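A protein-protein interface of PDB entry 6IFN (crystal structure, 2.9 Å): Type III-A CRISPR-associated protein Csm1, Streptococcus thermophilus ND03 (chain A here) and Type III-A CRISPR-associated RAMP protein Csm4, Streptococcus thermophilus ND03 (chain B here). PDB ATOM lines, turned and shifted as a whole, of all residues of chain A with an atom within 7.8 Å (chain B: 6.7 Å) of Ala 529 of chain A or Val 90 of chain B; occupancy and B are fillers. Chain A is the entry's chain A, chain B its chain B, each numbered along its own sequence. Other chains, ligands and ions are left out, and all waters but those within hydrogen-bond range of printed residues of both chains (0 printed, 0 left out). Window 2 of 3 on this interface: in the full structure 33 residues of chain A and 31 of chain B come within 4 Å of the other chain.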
ATOM      1  N   PHE A 114     -28.195 -13.034   4.830  1.00  0.00           N
ATOM      2  CA  PHE A 114     -27.354 -11.869   4.755  1.00  0.00           C
ATOM      3  C   PHE A 114     -27.304 -11.206   6.137  1.00  0.00           C
ATOM      4  O   PHE A 114     -28.341 -10.956   6.737  1.00  0.00           O
ATOM      5  CB  PHE A 114     -27.896 -10.897   3.709  1.00  0.00           C
ATOM      6  CG  PHE A 114     -27.023  -9.693   3.470  1.00  0.00           C
ATOM      7  CD1 PHE A 114     -27.031  -8.631   4.366  1.00  0.00           C
ATOM      8  CD2 PHE A 114     -26.210  -9.625   2.351  1.00  0.00           C
ATOM      9  CE1 PHE A 114     -26.230  -7.520   4.146  1.00  0.00           C
ATOM     10  CE2 PHE A 114     -25.407  -8.517   2.144  1.00  0.00           C
ATOM     11  CZ  PHE A 114     -25.413  -7.468   3.039  1.00  0.00           C
ATOM     12  N   GLY A 115     -26.097 -10.943   6.634  1.00  0.00           N
ATOM     13  CA  GLY A 115     -25.913 -10.205   7.904  1.00  0.00           C
ATOM     14  C   GLY A 115     -26.421 -10.955   9.128  1.00  0.00           C
ATOM     15  O   GLY A 115     -26.342 -12.167   9.199  1.00  0.00           O
ATOM     16  N   PRO A 360     -12.914 -18.783   4.066  1.00  0.00           N
ATOM     17  CA  PRO A 360     -12.838 -17.335   4.288  1.00  0.00           C
ATOM     18  C   PRO A 360     -11.968 -16.658   3.213  1.00  0.00           C
ATOM     19  O   PRO A 360     -12.473 -15.835   2.424  1.00  0.00           O
ATOM     20  CB  PRO A 360     -12.235 -17.183   5.696  1.00  0.00           C
ATOM     21  CG  PRO A 360     -11.568 -18.515   5.974  1.00  0.00           C
ATOM     22  CD  PRO A 360     -12.403 -19.536   5.222  1.00  0.00           C
ATOM     23  N   TYR A 363     -12.832 -17.790  -1.226  1.00  0.00           N
ATOM     24  CA  TYR A 363     -13.875 -17.171  -2.050  1.00  0.00           C
ATOM     25  C   TYR A 363     -13.558 -15.686  -2.305  1.00  0.00           C
ATOM     26  O   TYR A 363     -13.803 -15.175  -3.413  1.00  0.00           O
ATOM     27  CB  TYR A 363     -15.270 -17.311  -1.446  1.00  0.00           C
ATOM     28  CG  TYR A 363     -16.300 -16.515  -2.209  1.00  0.00           C
ATOM     29  CD1 TYR A 363     -16.433 -16.661  -3.585  1.00  0.00           C
ATOM     30  CD2 TYR A 363     -17.114 -15.585  -1.571  1.00  0.00           C
ATOM     31  CE1 TYR A 363     -17.354 -15.914  -4.303  1.00  0.00           C
ATOM     32  CE2 TYR A 363     -18.049 -14.838  -2.272  1.00  0.00           C
ATOM     33  CZ  TYR A 363     -18.165 -15.004  -3.641  1.00  0.00           C
ATOM     34  OH  TYR A 363     -19.080 -14.271  -4.330  1.00  0.00           O
ATOM     35  N   ARG A 364     -13.023 -14.990  -1.291  1.00  0.00           N
ATOM     36  CA  ARG A 364     -12.687 -13.574  -1.439  1.00  0.00           C
ATOM     37  C   ARG A 364     -11.483 -13.446  -2.384  1.00  0.00           C
ATOM     38  O   ARG A 364     -11.432 -12.524  -3.169  1.00  0.00           O
ATOM     39  CB  ARG A 364     -12.425 -12.898  -0.086  1.00  0.00           C
ATOM     40  N   GLN A 368      -9.967 -11.205  -5.865  1.00  0.00           N
ATOM     41  CA  GLN A 368      -8.906 -10.286  -5.513  1.00  0.00           C
ATOM     42  C   GLN A 368      -7.814 -10.292  -6.598  1.00  0.00           C
ATOM     43  O   GLN A 368      -7.145  -9.277  -6.787  1.00  0.00           O
ATOM     44  CB  GLN A 368      -8.361 -10.609  -4.120  1.00  0.00           C
ATOM     45  CG  GLN A 368      -7.698  -9.437  -3.413  1.00  0.00           C
ATOM     46  CD  GLN A 368      -8.102  -9.364  -1.963  1.00  0.00           C
ATOM     47  OE1 GLN A 368      -7.914 -10.300  -1.182  1.00  0.00           O
ATOM     48  NE2 GLN A 368      -8.690  -8.236  -1.600  1.00  0.00           N
ATOM     49  N   ASP A 522     -21.451   0.404   1.571  1.00  0.00           N
ATOM     50  CA  ASP A 522     -20.567  -0.695   1.708  1.00  0.00           C
ATOM     51  C   ASP A 522     -21.058  -1.848   0.823  1.00  0.00           C
ATOM     52  O   ASP A 522     -20.995  -3.001   1.229  1.00  0.00           O
ATOM     53  CB  ASP A 522     -20.454  -1.065   3.182  1.00  0.00           C
ATOM     54  CG  ASP A 522     -20.320   0.158   4.073  1.00  0.00           C
ATOM     55  OD1 ASP A 522     -19.340   0.930   3.900  1.00  0.00           O
ATOM     56  OD2 ASP A 522     -21.216   0.354   4.921  1.00  0.00           O
ATOM     57  N   LEU A 523     -21.545  -1.510  -0.381  1.00  0.00           N
ATOM     58  CA  LEU A 523     -22.045  -2.468  -1.398  1.00  0.00           C
ATOM     59  C   LEU A 523     -20.967  -3.510  -1.698  1.00  0.00           C
ATOM     60  O   LEU A 523     -21.250  -4.702  -1.682  1.00  0.00           O
ATOM     61  CB  LEU A 523     -22.440  -1.705  -2.669  1.00  0.00           C
ATOM     62  CG  LEU A 523     -22.999  -2.540  -3.819  1.00  0.00           C
ATOM     63  CD1 LEU A 523     -24.355  -3.100  -3.478  1.00  0.00           C
ATOM     64  CD2 LEU A 523     -23.116  -1.715  -5.089  1.00  0.00           C
ATOM     65  N   GLY A 524     -19.732  -3.044  -1.931  1.00  0.00           N
ATOM     66  CA  GLY A 524     -18.585  -3.944  -2.110  1.00  0.00           C
ATOM     67  C   GLY A 524     -18.520  -5.021  -1.038  1.00  0.00           C
ATOM     68  O   GLY A 524     -18.418  -6.216  -1.321  1.00  0.00           O
ATOM     69  N   ALA A 525     -18.626  -4.572   0.212  1.00  0.00           N
ATOM     70  CA  ALA A 525     -18.589  -5.443   1.370  1.00  0.00           C
ATOM     71  C   ALA A 525     -19.755  -6.448   1.352  1.00  0.00           C
ATOM     72  O   ALA A 525     -19.621  -7.565   1.836  1.00  0.00           O
ATOM     73  CB  ALA A 525     -18.599  -4.603   2.628  1.00  0.00           C
ATOM     74  N   ALA A 526     -20.910  -6.044   0.825  1.00  0.00           N
ATOM     75  CA  ALA A 526     -22.052  -6.913   0.800  1.00  0.00           C
ATOM     76  C   ALA A 526     -21.804  -8.020  -0.216  1.00  0.00           C
ATOM     77  O   ALA A 526     -22.014  -9.181   0.070  1.00  0.00           O
ATOM     78  CB  ALA A 526     -23.294  -6.130   0.454  1.00  0.00           C
ATOM     79  N   PHE A 527     -21.369  -7.621  -1.411  1.00  0.00           N
ATOM     80  CA  PHE A 527     -21.206  -8.531  -2.541  1.00  0.00           C
ATOM     81  C   PHE A 527     -20.214  -9.634  -2.146  1.00  0.00           C
ATOM     82  O   PHE A 527     -20.445 -10.816  -2.417  1.00  0.00           O
ATOM     83  CB  PHE A 527     -20.820  -7.724  -3.785  1.00  0.00           C
ATOM     84  CG  PHE A 527     -20.451  -8.515  -5.014  1.00  0.00           C
ATOM     85  CD1 PHE A 527     -21.294  -9.487  -5.527  1.00  0.00           C
ATOM     86  CD2 PHE A 527     -19.276  -8.237  -5.710  1.00  0.00           C
ATOM     87  CE1 PHE A 527     -20.953 -10.184  -6.685  1.00  0.00           C
ATOM     88  CE2 PHE A 527     -18.940  -8.932  -6.869  1.00  0.00           C
ATOM     89  CZ  PHE A 527     -19.778  -9.912  -7.354  1.00  0.00           C
ATOM     90  N   MET A 528     -19.150  -9.250  -1.438  1.00  0.00           N
ATOM     91  CA  MET A 528     -18.024 -10.135  -1.210  1.00  0.00           C
ATOM     92  C   MET A 528     -18.251 -10.936   0.074  1.00  0.00           C
ATOM     93  O   MET A 528     -18.316 -12.159   0.016  1.00  0.00           O
ATOM     94  CB  MET A 528     -16.712  -9.348  -1.147  1.00  0.00           C
ATOM     95  CG  MET A 528     -16.444  -8.551  -2.424  1.00  0.00           C
ATOM     96  SD  MET A 528     -14.711  -8.455  -2.926  1.00  0.00           S
ATOM     97  CE  MET A 528     -13.968  -7.660  -1.497  1.00  0.00           C
ATOM     98  N   ALA A 529     -18.408 -10.247   1.214  1.00  0.00           N
ATOM     99  CA  ALA A 529     -18.762 -10.908   2.485  1.00  0.00           C
ATOM    100  C   ALA A 529     -19.905 -10.174   3.221  1.00  0.00           C
ATOM    101  O   ALA A 529     -19.686  -9.284   4.039  1.00  0.00           O
ATOM    102  CB  ALA A 529     -17.529 -11.024   3.337  1.00  0.00           C
ATOM    103  N   GLY A 530     -21.144 -10.549   2.900  1.00  0.00           N
ATOM    104  CA  GLY A 530     -22.306 -10.190   3.670  1.00  0.00           C
ATOM    105  C   GLY A 530     -22.988 -11.439   4.174  1.00  0.00           C
ATOM    106  O   GLY A 530     -23.846 -11.369   5.044  1.00  0.00           O
ATOM    107  N   PHE A 531     -22.590 -12.589   3.621  1.00  0.00           N
ATOM    108  CA  PHE A 531     -23.206 -13.868   3.930  1.00  0.00           C
ATOM    109  C   PHE A 531     -22.316 -14.677   4.889  1.00  0.00           C
ATOM    110  O   PHE A 531     -22.637 -15.829   5.259  1.00  0.00           O
ATOM    111  CB  PHE A 531     -23.506 -14.605   2.627  1.00  0.00           C
ATOM    112  CG  PHE A 531     -24.300 -13.801   1.627  1.00  0.00           C
ATOM    113  CD1 PHE A 531     -25.623 -13.474   1.866  1.00  0.00           C
ATOM    114  CD2 PHE A 531     -23.734 -13.382   0.437  1.00  0.00           C
ATOM    115  CE1 PHE A 531     -26.365 -12.765   0.936  1.00  0.00           C
ATOM    116  CE2 PHE A 531     -24.484 -12.683  -0.496  1.00  0.00           C
ATOM    117  CZ  PHE A 531     -25.794 -12.367  -0.241  1.00  0.00           C
ATOM    118  N   SER A 532     -21.220 -14.059   5.336  1.00  0.00           N
ATOM    119  CA  SER A 532     -20.235 -14.736   6.159  1.00  0.00           C
ATOM    120  C   SER A 532     -20.653 -14.720   7.638  1.00  0.00           C
ATOM    121  O   SER A 532     -20.368 -15.685   8.365  1.00  0.00           O
ATOM    122  CB  SER A 532     -18.878 -14.126   5.955  1.00  0.00           C
ATOM    123  OG  SER A 532     -18.977 -12.713   5.945  1.00  0.00           O
ATOM    124  N   GLN A 533     -21.335 -13.647   8.074  1.00  0.00           N
ATOM    125  CA  GLN A 533     -21.739 -13.501   9.484  1.00  0.00           C
ATOM    126  C   GLN A 533     -22.551 -14.741   9.882  1.00  0.00           C
ATOM    127  O   GLN A 533     -22.090 -15.556  10.642  1.00  0.00           O
ATOM    128  CB  GLN A 533     -22.479 -12.174   9.693  1.00  0.00           C
ATOM    129  CG  GLN A 533     -22.689 -11.789  11.161  1.00  0.00           C
ATOM    130  CD  GLN A 533     -23.075 -10.336  11.368  1.00  0.00           C
ATOM    131  OE1 GLN A 533     -22.793  -9.468  10.539  1.00  0.00           O
ATOM    132  NE2 GLN A 533     -23.717 -10.040  12.489  1.00  0.00           N
ATOM    133  N   SER A 540     -21.456 -18.154   2.216  1.00  0.00           N
ATOM    134  CA  SER A 540     -20.757 -17.324   1.242  1.00  0.00           C
ATOM    135  C   SER A 540     -20.367 -18.191   0.039  1.00  0.00           C
ATOM    136  O   SER A 540     -19.358 -18.869   0.076  1.00  0.00           O
ATOM    137  CB  SER A 540     -19.567 -16.649   1.868  1.00  0.00           C
ATOM    138  OG  SER A 540     -19.971 -15.781   2.917  1.00  0.00           O
ATOM    139  N   SER A 545     -23.866 -14.738  -4.098  1.00  0.00           N
ATOM    140  CA  SER A 545     -23.447 -13.404  -4.509  1.00  0.00           C
ATOM    141  C   SER A 545     -24.064 -13.025  -5.866  1.00  0.00           C
ATOM    142  O   SER A 545     -24.540 -11.903  -6.025  1.00  0.00           O
ATOM    143  CB  SER A 545     -21.945 -13.297  -4.511  1.00  0.00           C
ATOM    144  OG  SER A 545     -21.385 -14.146  -5.500  1.00  0.00           O
ATOM    145  N   VAL B  88      -8.372  -7.733   9.574  1.00  0.00           N
ATOM    146  CA  VAL B  88      -9.716  -7.148   9.803  1.00  0.00           C
ATOM    147  C   VAL B  88     -10.683  -7.575   8.690  1.00  0.00           C
ATOM    148  O   VAL B  88     -10.272  -7.937   7.575  1.00  0.00           O
ATOM    149  CB  VAL B  88      -9.698  -5.608   9.917  1.00  0.00           C
ATOM    150  CG1 VAL B  88      -9.539  -5.132  11.355  1.00  0.00           C
ATOM    151  CG2 VAL B  88      -8.655  -4.970   9.010  1.00  0.00           C
ATOM    152  N   ASP B  89     -11.978  -7.472   9.016  1.00  0.00           N
ATOM    153  CA  ASP B  89     -13.111  -7.771   8.125  1.00  0.00           C
ATOM    154  C   ASP B  89     -13.031  -6.901   6.861  1.00  0.00           C
ATOM    155  O   ASP B  89     -12.204  -5.985   6.770  1.00  0.00           O
ATOM    156  CB  ASP B  89     -14.444  -7.513   8.833  1.00  0.00           C
ATOM    157  CG  ASP B  89     -14.715  -6.033   9.019  1.00  0.00           C
ATOM    158  OD1 ASP B  89     -13.778  -5.331   9.447  1.00  0.00           O
ATOM    159  OD2 ASP B  89     -15.838  -5.591   8.699  1.00  0.00           O
ATOM    160  N   VAL B  90     -13.923  -7.176   5.906  1.00  0.00           N
ATOM    161  CA  VAL B  90     -13.825  -6.603   4.581  1.00  0.00           C
ATOM    162  C   VAL B  90     -14.329  -5.151   4.607  1.00  0.00           C
ATOM    163  O   VAL B  90     -13.738  -4.259   3.983  1.00  0.00           O
ATOM    164  CB  VAL B  90     -14.574  -7.429   3.523  1.00  0.00           C
ATOM    165  CG1 VAL B  90     -14.179  -6.975   2.132  1.00  0.00           C
ATOM    166  CG2 VAL B  90     -14.342  -8.921   3.668  1.00  0.00           C
ATOM    167  N   LYS B  91     -15.420  -4.905   5.328  1.00  0.00           N
ATOM    168  CA  LYS B  91     -15.998  -3.584   5.321  1.00  0.00           C
ATOM    169  C   LYS B  91     -14.930  -2.556   5.747  1.00  0.00           C
ATOM    170  O   LYS B  91     -14.894  -1.443   5.203  1.00  0.00           O
ATOM    171  CB  LYS B  91     -17.259  -3.551   6.190  1.00  0.00           C
ATOM    172  CG  LYS B  91     -18.109  -2.305   5.979  1.00  0.00           C
ATOM    173  CD  LYS B  91     -19.283  -2.150   6.901  1.00  0.00           C
ATOM    174  CE  LYS B  91     -20.562  -2.765   6.364  1.00  0.00           C
ATOM    175  NZ  LYS B  91     -21.764  -2.020   6.819  1.00  0.00           N
ATOM    176  N   GLU B  92     -14.070  -2.925   6.713  1.00  0.00           N
ATOM    177  CA  GLU B  92     -13.031  -2.027   7.248  1.00  0.00           C
ATOM    178  C   GLU B  92     -11.917  -1.854   6.221  1.00  0.00           C
ATOM    179  O   GLU B  92     -11.550  -0.731   5.891  1.00  0.00           O
ATOM    180  CB  GLU B  92     -12.431  -2.537   8.558  1.00  0.00           C
ATOM    181  CG  GLU B  92     -13.059  -1.895   9.779  1.00  0.00           C
ATOM    182  CD  GLU B  92     -13.150  -0.385   9.650  1.00  0.00           C
ATOM    183  OE1 GLU B  92     -12.102   0.224   9.363  1.00  0.00           O
ATOM    184  OE2 GLU B  92     -14.271   0.172   9.782  1.00  0.00           O
ATOM    185  N   VAL B  93     -11.389  -2.968   5.718  1.00  0.00           N
ATOM    186  CA  VAL B  93     -10.367  -2.897   4.690  1.00  0.00           C
ATOM    187  C   VAL B  93     -10.818  -1.938   3.575  1.00  0.00           C
ATOM    188  O   VAL B  93     -10.029  -1.158   3.090  1.00  0.00           O
ATOM    189  CB  VAL B  93     -10.017  -4.300   4.156  1.00  0.00           C
ATOM    190  CG1 VAL B  93      -9.598  -4.307   2.688  1.00  0.00           C
ATOM    191  CG2 VAL B  93      -8.966  -4.958   5.046  1.00  0.00           C
ATOM    192  N   ARG B  94     -12.083  -2.007   3.168  1.00  0.00           N
ATOM    193  CA  ARG B  94     -12.529  -1.247   1.994  1.00  0.00           C
ATOM    194  C   ARG B  94     -12.777   0.212   2.377  1.00  0.00           C
ATOM    195  O   ARG B  94     -12.572   1.092   1.546  1.00  0.00           O
ATOM    196  CB  ARG B  94     -13.761  -1.875   1.333  1.00  0.00           C
ATOM    197  CG  ARG B  94     -13.458  -3.212   0.670  1.00  0.00           C
ATOM    198  CD  ARG B  94     -14.684  -3.797   0.015  1.00  0.00           C
ATOM    199  NE  ARG B  94     -15.026  -3.094  -1.205  1.00  0.00           N
ATOM    200  CZ  ARG B  94     -14.761  -3.537  -2.426  1.00  0.00           C
ATOM    201  NH1 ARG B  94     -14.218  -4.731  -2.605  1.00  0.00           N
ATOM    202  NH2 ARG B  94     -15.056  -2.775  -3.461  1.00  0.00           N
ATOM    203  N   ARG B  95     -13.191   0.467   3.624  1.00  0.00           N
ATOM    204  CA  ARG B  95     -13.373   1.851   4.069  1.00  0.00           C
ATOM    205  C   ARG B  95     -12.010   2.550   4.054  1.00  0.00           C
ATOM    206  O   ARG B  95     -11.901   3.634   3.501  1.00  0.00           O
ATOM    207  CB  ARG B  95     -14.051   1.946   5.439  1.00  0.00           C
ATOM    208  CG  ARG B  95     -15.556   1.712   5.388  1.00  0.00           C
ATOM    209  CD  ARG B  95     -16.283   2.084   6.669  1.00  0.00           C
ATOM    210  NE  ARG B  95     -17.638   1.547   6.724  1.00  0.00           N
ATOM    211  CZ  ARG B  95     -18.578   1.958   7.566  1.00  0.00           C
ATOM    212  NH1 ARG B  95     -18.281   2.816   8.532  1.00  0.00           N
ATOM    213  NH2 ARG B  95     -19.818   1.528   7.422  1.00  0.00           N
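Of the 8 printed residues of chain B, 4 touch a printed residue of chain A.
Printed residues of chain A that touch a printed residue of chain B: Asp 522, Gly 524, Ala 525, Met 528 and Ala 529.
Hydrophobic or aromatic side chains of chain A within 4 Å of the printed part of chain B: Ala 525, Met 528 and Ala 529.
Among the printed residues, 7 pairs touch across the chains.
Among the printed residues, Asp or Glu carboxylates within 4 Å of a Lys or Arg side-chain nitrogen of the other chain: Asp 522 of chain A with Lys 91 of chain B (3.1 Å) and Asp 522 of chain A with Arg 95 of chain B (3.1 Å).
Among the printed residues, pairs that only touch across the chains: Gly 524 of chain A with Arg 94 of chain B (3.8 Å), Ala 525 of chain A with Lys 91 of chain B (3.9 Å), Met 528 of chain A with Val 90 of chain B (3.7 Å) and Ala 529 of chain A with Val 90 of chain B (3.8 Å).
OD2 of Asp 89 of chain B sits at hydrogen-bond distance from N of Lys 91 of chain B (3.5 Å).
Printed residues of chain B within 4 Å of Asp 522 of chain A: Lys 91 and Arg 95.
Of the printed residues of chain B, Gly 524 of chain A touches Arg 94.
Of the printed residues of chain B, Ala 525 of chain A touches Lys 91.
Phe 527 of chain A touches none of the printed residues of chain B.
Of chain B, only Val 90 comes within 4 Å of Ala 529 of chain A.
Val 90 of chain B touches just these residues of chain A: Met 528 (3.7 Å) and Ala 529 (3.8 Å).
Of the printed residues of chain A, Arg 94 of chain B touches Gly 524 (3.8 Å) and Met 528 (3.1 Å).
Printed residues of chain A within 4 Å of Arg 95 of chain B: Asp 522 (3.1 Å).
The nearest residue of chain B that does not touch Ala 529 of chain A is Lys 91 of chain B (6.2 Å).
The nearest residue of chain A that does not touch Val 90 of chain B is Ala 525 of chain A (4.7 Å).
The side-chain carboxylate (OD2) of Asp 522 of chain A lies within salt-bridge range of the side-chain amino group (NZ) of Lys 91 of chain B.
The side-chain carboxylate (OD2) of Asp 522 of chain A lies within salt-bridge range of the guanidinium group (NH2) of Arg 95 of chain B (3.1 Å).
NH1 of Arg 94 of chain B sits close to SD of Met 528 of chain A (3.8 Å).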
